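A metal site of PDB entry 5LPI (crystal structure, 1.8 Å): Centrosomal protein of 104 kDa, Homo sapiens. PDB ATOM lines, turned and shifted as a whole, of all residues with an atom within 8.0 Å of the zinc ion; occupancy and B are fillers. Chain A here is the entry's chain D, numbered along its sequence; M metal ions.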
ATOM      1  N   LEU A  12       1.633  12.588 -14.685  1.00  0.00           N
ATOM      2  CA  LEU A  12       0.407  12.727 -13.921  1.00  0.00           C
ATOM      3  C   LEU A  12      -0.045  11.386 -13.368  1.00  0.00           C
ATOM      4  O   LEU A  12      -0.131  10.402 -14.115  1.00  0.00           O
ATOM      5  CB  LEU A  12      -0.703  13.332 -14.782  1.00  0.00           C
ATOM      6  CG  LEU A  12      -2.125  13.202 -14.228  1.00  0.00           C
ATOM      7  CD1 LEU A  12      -2.412  14.272 -13.176  1.00  0.00           C
ATOM      8  CD2 LEU A  12      -3.142  13.255 -15.373  1.00  0.00           C
ATOM      9  N   CYS A  13      -0.366  11.336 -12.082  1.00  0.00           N
ATOM     10  CA  CYS A  13      -1.097  10.195 -11.520  1.00  0.00           C
ATOM     11  C   CYS A  13      -2.590  10.418 -11.755  1.00  0.00           C
ATOM     12  O   CYS A  13      -3.195  11.283 -11.124  1.00  0.00           O
ATOM     13  CB  CYS A  13      -0.823  10.042 -10.034  1.00  0.00           C
ATOM     14  SG  CYS A  13      -1.784   8.693  -9.269  1.00  0.00           S
ATOM     15  N   ILE A  14      -3.186   9.617 -12.635  1.00  0.00           N
ATOM     16  CA  ILE A  14      -4.613   9.767 -12.909  1.00  0.00           C
ATOM     17  C   ILE A  14      -5.499   9.397 -11.734  1.00  0.00           C
ATOM     18  O   ILE A  14      -6.697   9.721 -11.757  1.00  0.00           O
ATOM     19  CB  ILE A  14      -5.025   8.932 -14.129  1.00  0.00           C
ATOM     20  CG1 ILE A  14      -4.840   7.453 -13.844  1.00  0.00           C
ATOM     21  CG2 ILE A  14      -4.207   9.328 -15.365  1.00  0.00           C
ATOM     22  CD1 ILE A  14      -5.426   6.568 -14.892  1.00  0.00           C
ATOM     23  N   PHE A  15      -4.960   8.756 -10.702  1.00  0.00           N
ATOM     24  CA  PHE A  15      -5.792   8.368  -9.566  1.00  0.00           C
ATOM     25  C   PHE A  15      -5.930   9.478  -8.542  1.00  0.00           C
ATOM     26  O   PHE A  15      -7.049   9.813  -8.143  1.00  0.00           O
ATOM     27  CB  PHE A  15      -5.229   7.097  -8.916  1.00  0.00           C
ATOM     28  CG  PHE A  15      -5.102   5.988  -9.877  1.00  0.00           C
ATOM     29  CD1 PHE A  15      -6.224   5.375 -10.390  1.00  0.00           C
ATOM     30  CD2 PHE A  15      -3.850   5.599 -10.339  1.00  0.00           C
ATOM     31  CE1 PHE A  15      -6.125   4.363 -11.312  1.00  0.00           C
ATOM     32  CE2 PHE A  15      -3.735   4.576 -11.264  1.00  0.00           C
ATOM     33  CZ  PHE A  15      -4.876   3.962 -11.755  1.00  0.00           C
ATOM     34  N   CYS A  16      -4.824  10.049  -8.096  1.00  0.00           N
ATOM     35  CA  CYS A  16      -4.908  11.130  -7.133  1.00  0.00           C
ATOM     36  C   CYS A  16      -4.732  12.511  -7.755  1.00  0.00           C
ATOM     37  O   CYS A  16      -4.938  13.520  -7.057  1.00  0.00           O
ATOM     38  CB  CYS A  16      -3.861  10.943  -6.023  1.00  0.00           C
ATOM     39  SG  CYS A  16      -2.167  11.229  -6.527  1.00  0.00           S
ATOM     40  N   GLY A  17      -4.400  12.578  -9.039  1.00  0.00           N
ATOM     41  CA  GLY A  17      -4.276  13.856  -9.724  1.00  0.00           C
ATOM     42  C   GLY A  17      -2.920  14.527  -9.590  1.00  0.00           C
ATOM     43  O   GLY A  17      -2.639  15.461 -10.338  1.00  0.00           O
ATOM     44  N   GLU A  18      -2.067  14.067  -8.671  1.00  0.00           N
ATOM     45  CA  GLU A  18      -0.784  14.727  -8.451  1.00  0.00           C
ATOM     46  C   GLU A  18       0.049  14.712  -9.716  1.00  0.00           C
ATOM     47  O   GLU A  18       0.033  13.757 -10.495  1.00  0.00           O
ATOM     48  CB  GLU A  18      -0.007  14.020  -7.330  1.00  0.00           C
ATOM     49  CG  GLU A  18      -0.371  14.460  -5.918  1.00  0.00           C
ATOM     50  CD  GLU A  18       0.567  13.885  -4.873  1.00  0.00           C
ATOM     51  OE1 GLU A  18       1.692  13.471  -5.245  1.00  0.00           O
ATOM     52  OE2 GLU A  18       0.175  13.831  -3.693  1.00  0.00           O
ATOM     53  N   ARG A  19       0.793  15.794  -9.913  1.00  0.00           N
ATOM     54  CA  ARG A  19       1.800  15.895 -10.961  1.00  0.00           C
ATOM     55  C   ARG A  19       3.160  16.093 -10.307  1.00  0.00           C
ATOM     56  O   ARG A  19       3.273  16.757  -9.280  1.00  0.00           O
ATOM     57  CB  ARG A  19       1.491  17.060 -11.918  1.00  0.00           C
ATOM     58  CG  ARG A  19       0.412  16.760 -12.943  1.00  0.00           C
ATOM     59  CD  ARG A  19       0.129  17.984 -13.831  1.00  0.00           C
ATOM     60  NE  ARG A  19      -1.064  17.782 -14.656  1.00  0.00           N
ATOM     61  CZ  ARG A  19      -1.060  17.116 -15.806  1.00  0.00           C
ATOM     62  NH1 ARG A  19       0.071  16.589 -16.269  1.00  0.00           N
ATOM     63  NH2 ARG A  19      -2.179  16.971 -16.496  1.00  0.00           N
ATOM     64  N   PHE A  23       7.362  11.687 -11.542  1.00  0.00           N
ATOM     65  CA  PHE A  23       6.359  10.733 -12.022  1.00  0.00           C
ATOM     66  C   PHE A  23       6.637  10.315 -13.453  1.00  0.00           C
ATOM     67  O   PHE A  23       5.759  10.429 -14.326  1.00  0.00           O
ATOM     68  CB  PHE A  23       4.940  11.305 -11.941  1.00  0.00           C
ATOM     69  CG  PHE A  23       4.393  11.340 -10.558  1.00  0.00           C
ATOM     70  CD1 PHE A  23       5.059  10.713  -9.526  1.00  0.00           C
ATOM     71  CD2 PHE A  23       3.197  12.000 -10.291  1.00  0.00           C
ATOM     72  CE1 PHE A  23       4.561  10.763  -8.237  1.00  0.00           C
ATOM     73  CE2 PHE A  23       2.693  12.043  -9.013  1.00  0.00           C
ATOM     74  CZ  PHE A  23       3.372  11.421  -7.991  1.00  0.00           C
ATOM     75  N   LEU A  28       5.960   6.475 -11.533  1.00  0.00           N
ATOM     76  CA  LEU A  28       4.541   6.231 -11.273  1.00  0.00           C
ATOM     77  C   LEU A  28       4.314   4.840 -10.699  1.00  0.00           C
ATOM     78  O   LEU A  28       3.467   4.666  -9.810  1.00  0.00           O
ATOM     79  CB  LEU A  28       3.718   6.413 -12.558  1.00  0.00           C
ATOM     80  CG  LEU A  28       3.296   7.828 -12.942  1.00  0.00           C
ATOM     81  CD1 LEU A  28       2.704   7.864 -14.346  1.00  0.00           C
ATOM     82  CD2 LEU A  28       2.291   8.384 -11.937  1.00  0.00           C
ATOM     83  N   HIS A  31       5.107   5.144  -7.181  1.00  0.00           N
ATOM     84  CA  HIS A  31       3.999   5.906  -6.610  1.00  0.00           C
ATOM     85  C   HIS A  31       2.809   5.020  -6.265  1.00  0.00           C
ATOM     86  O   HIS A  31       2.296   5.062  -5.149  1.00  0.00           O
ATOM     87  CB  HIS A  31       3.594   7.006  -7.609  1.00  0.00           C
ATOM     88  CG  HIS A  31       2.453   7.858  -7.122  1.00  0.00           C
ATOM     89  ND1 HIS A  31       2.568   8.707  -6.054  1.00  0.00           N
ATOM     90  CD2 HIS A  31       1.184   7.973  -7.570  1.00  0.00           C
ATOM     91  CE1 HIS A  31       1.415   9.324  -5.859  1.00  0.00           C
ATOM     92  NE2 HIS A  31       0.554   8.895  -6.764  1.00  0.00           N
ATOM     93  N   TYR A  32       2.343   4.204  -7.222  1.00  0.00           N
ATOM     94  CA  TYR A  32       1.192   3.350  -6.967  1.00  0.00           C
ATOM     95  C   TYR A  32       1.499   2.316  -5.887  1.00  0.00           C
ATOM     96  O   TYR A  32       0.641   1.989  -5.063  1.00  0.00           O
ATOM     97  CB  TYR A  32       0.739   2.616  -8.227  1.00  0.00           C
ATOM     98  CG  TYR A  32       0.551   3.440  -9.497  1.00  0.00           C
ATOM     99  CD1 TYR A  32      -0.010   4.710  -9.475  1.00  0.00           C
ATOM    100  CD2 TYR A  32       0.919   2.909 -10.732  1.00  0.00           C
ATOM    101  CE1 TYR A  32      -0.178   5.441 -10.661  1.00  0.00           C
ATOM    102  CE2 TYR A  32       0.753   3.627 -11.920  1.00  0.00           C
ATOM    103  CZ  TYR A  32       0.200   4.900 -11.868  1.00  0.00           C
ATOM    104  OH  TYR A  32       0.044   5.611 -13.048  1.00  0.00           O
ATOM    105  N   HIS A  35       2.747   4.971  -2.377  1.00  0.00           N
ATOM    106  CA  HIS A  35       2.456   6.319  -1.899  1.00  0.00           C
ATOM    107  C   HIS A  35       1.063   6.834  -2.228  1.00  0.00           C
ATOM    108  O   HIS A  35       0.499   7.571  -1.419  1.00  0.00           O
ATOM    109  CB  HIS A  35       3.480   7.297  -2.457  1.00  0.00           C
ATOM    110  CG  HIS A  35       4.879   6.952  -2.080  1.00  0.00           C
ATOM    111  ND1 HIS A  35       5.305   6.947  -0.768  1.00  0.00           N
ATOM    112  CD2 HIS A  35       5.948   6.589  -2.825  1.00  0.00           C
ATOM    113  CE1 HIS A  35       6.580   6.584  -0.718  1.00  0.00           C
ATOM    114  NE2 HIS A  35       6.997   6.367  -1.956  1.00  0.00           N
ATOM    115  N   CYS A  36       0.491   6.511  -3.387  1.00  0.00           N
ATOM    116  CA  CYS A  36      -0.766   7.138  -3.802  1.00  0.00           C
ATOM    117  C   CYS A  36      -1.875   6.903  -2.787  1.00  0.00           C
ATOM    118  O   CYS A  36      -2.203   5.757  -2.457  1.00  0.00           O
ATOM    119  CB  CYS A  36      -1.204   6.597  -5.164  1.00  0.00           C
ATOM    120  SG  CYS A  36      -2.703   7.416  -5.829  1.00  0.00           S
ATOM    121  N   LEU A  37      -2.484   8.000  -2.300  1.00  0.00           N
ATOM    122  CA  LEU A  37      -3.512   7.889  -1.261  1.00  0.00           C
ATOM    123  C   LEU A  37      -4.803   7.254  -1.781  1.00  0.00           C
ATOM    124  O   LEU A  37      -5.619   6.806  -0.972  1.00  0.00           O
ATOM    125  CB  LEU A  37      -3.819   9.271  -0.674  1.00  0.00           C
ATOM    126  CG  LEU A  37      -2.663   9.946   0.059  1.00  0.00           C
ATOM    127  CD1 LEU A  37      -3.049  11.329   0.552  1.00  0.00           C
ATOM    128  CD2 LEU A  37      -2.183   9.092   1.214  1.00  0.00           C
ATOM    129  N   MET A  38      -5.006   7.210  -3.083  1.00  0.00           N
ATOM    130  CA  MET A  38      -6.237   6.647  -3.638  1.00  0.00           C
ATOM    131  C   MET A  38      -6.157   5.145  -3.866  1.00  0.00           C
ATOM    132  O   MET A  38      -7.178   4.521  -4.197  1.00  0.00           O
ATOM    133  CB  MET A  38      -6.581   7.349  -4.954  1.00  0.00           C
ATOM    134  CG  MET A  38      -6.741   8.862  -4.808  1.00  0.00           C
ATOM    135  SD  MET A  38      -8.174   9.296  -3.781  1.00  0.00           S
ATOM    136  CE  MET A  38      -9.469   8.506  -4.735  1.00  0.00           C
ATOM    137  N   LEU A  39      -4.991   4.564  -3.689  1.00  0.00           N
ATOM    138  CA  LEU A  39      -4.768   3.156  -3.966  1.00  0.00           C
ATOM    139  C   LEU A  39      -4.385   2.433  -2.688  1.00  0.00           C
ATOM    140  O   LEU A  39      -3.969   3.039  -1.690  1.00  0.00           O
ATOM    141  CB  LEU A  39      -3.670   2.962  -5.022  1.00  0.00           C
ATOM    142  CG  LEU A  39      -3.774   3.838  -6.271  1.00  0.00           C
ATOM    143  CD1 LEU A  39      -2.540   3.601  -7.174  1.00  0.00           C
ATOM    144  CD2 LEU A  39      -5.064   3.562  -7.057  1.00  0.00           C
ATOM    145  N   MET A 123      -8.181  11.595   0.738  1.00  0.00           N
ATOM    146  CA  MET A 123      -6.988  12.422   0.832  1.00  0.00           C
ATOM    147  C   MET A 123      -7.144  13.682   1.658  1.00  0.00           C
ATOM    148  O   MET A 123      -6.139  14.247   2.093  1.00  0.00           O
ATOM    149  CB  MET A 123      -6.540  12.832  -0.569  1.00  0.00           C
ATOM    150  CG  MET A 123      -6.524  11.671  -1.508  1.00  0.00           C
ATOM    151  SD  MET A 123      -5.544  12.044  -2.936  1.00  0.00           S
ATOM    152  CE  MET A 123      -6.651  12.937  -3.953  1.00  0.00           C
ATOM    153  N   ARG A 133      -2.139   4.682   4.089  1.00  0.00           N
ATOM    154  CA  ARG A 133      -1.118   5.504   3.455  1.00  0.00           C
ATOM    155  C   ARG A 133      -1.213   6.959   3.870  1.00  0.00           C
ATOM    156  O   ARG A 133      -0.352   7.749   3.491  1.00  0.00           O
ATOM    157  CB  ARG A 133      -1.192   5.414   1.930  1.00  0.00           C
ATOM    158  CG  ARG A 133      -0.842   4.047   1.393  1.00  0.00           C
ATOM    159  CD  ARG A 133      -0.995   3.992  -0.099  1.00  0.00           C
ATOM    160  NE  ARG A 133      -0.629   2.685  -0.628  1.00  0.00           N
ATOM    161  CZ  ARG A 133      -0.472   2.448  -1.915  1.00  0.00           C
ATOM    162  NH1 ARG A 133      -0.641   3.443  -2.781  1.00  0.00           N
ATOM    163  NH2 ARG A 133      -0.121   1.233  -2.325  1.00  0.00           N
HETATM  164 ZN    ZN M   1      -1.551   9.049  -7.053  1.00  0.00          ZN
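The side-chain sulfur of Cys 13 sits close to the backbone NH of Phe 15, 3.5 Å away. The side-chain sulfur of Cys 36 lies close to the backbone NH of Met 38, 3.6 Å away. N of Cys 13 sits at hydrogen-bond distance from O of Glu 18, at 2.9 Å. SG of Cys 16 sits close to N of Glu 18. The guanidinium group (NH1) of Arg 133 sits at hydrogen-bond distance from the backbone carbonyl oxygen (O) of Cys 36 (2.8 Å).
Four residues have an atom within 4 Å of the zinc ion: Cys 13, Cys 16, His 31 and Cys 36. The nearest printed residue that does not touch the zinc ion is Phe 15 (4.6 Å).
A ring nitrogen (NE2) of His 31 is bound to the zinc ion, 2.1 Å away. SG of Cys 13 is bound to the zinc ion (2.3 Å). SG of Cys 16 binds the zinc ion (2.3 Å). SG of Cys 36 binds the zinc ion, at 2.3 Å. The zinc ion has four donor atoms within binding distance.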
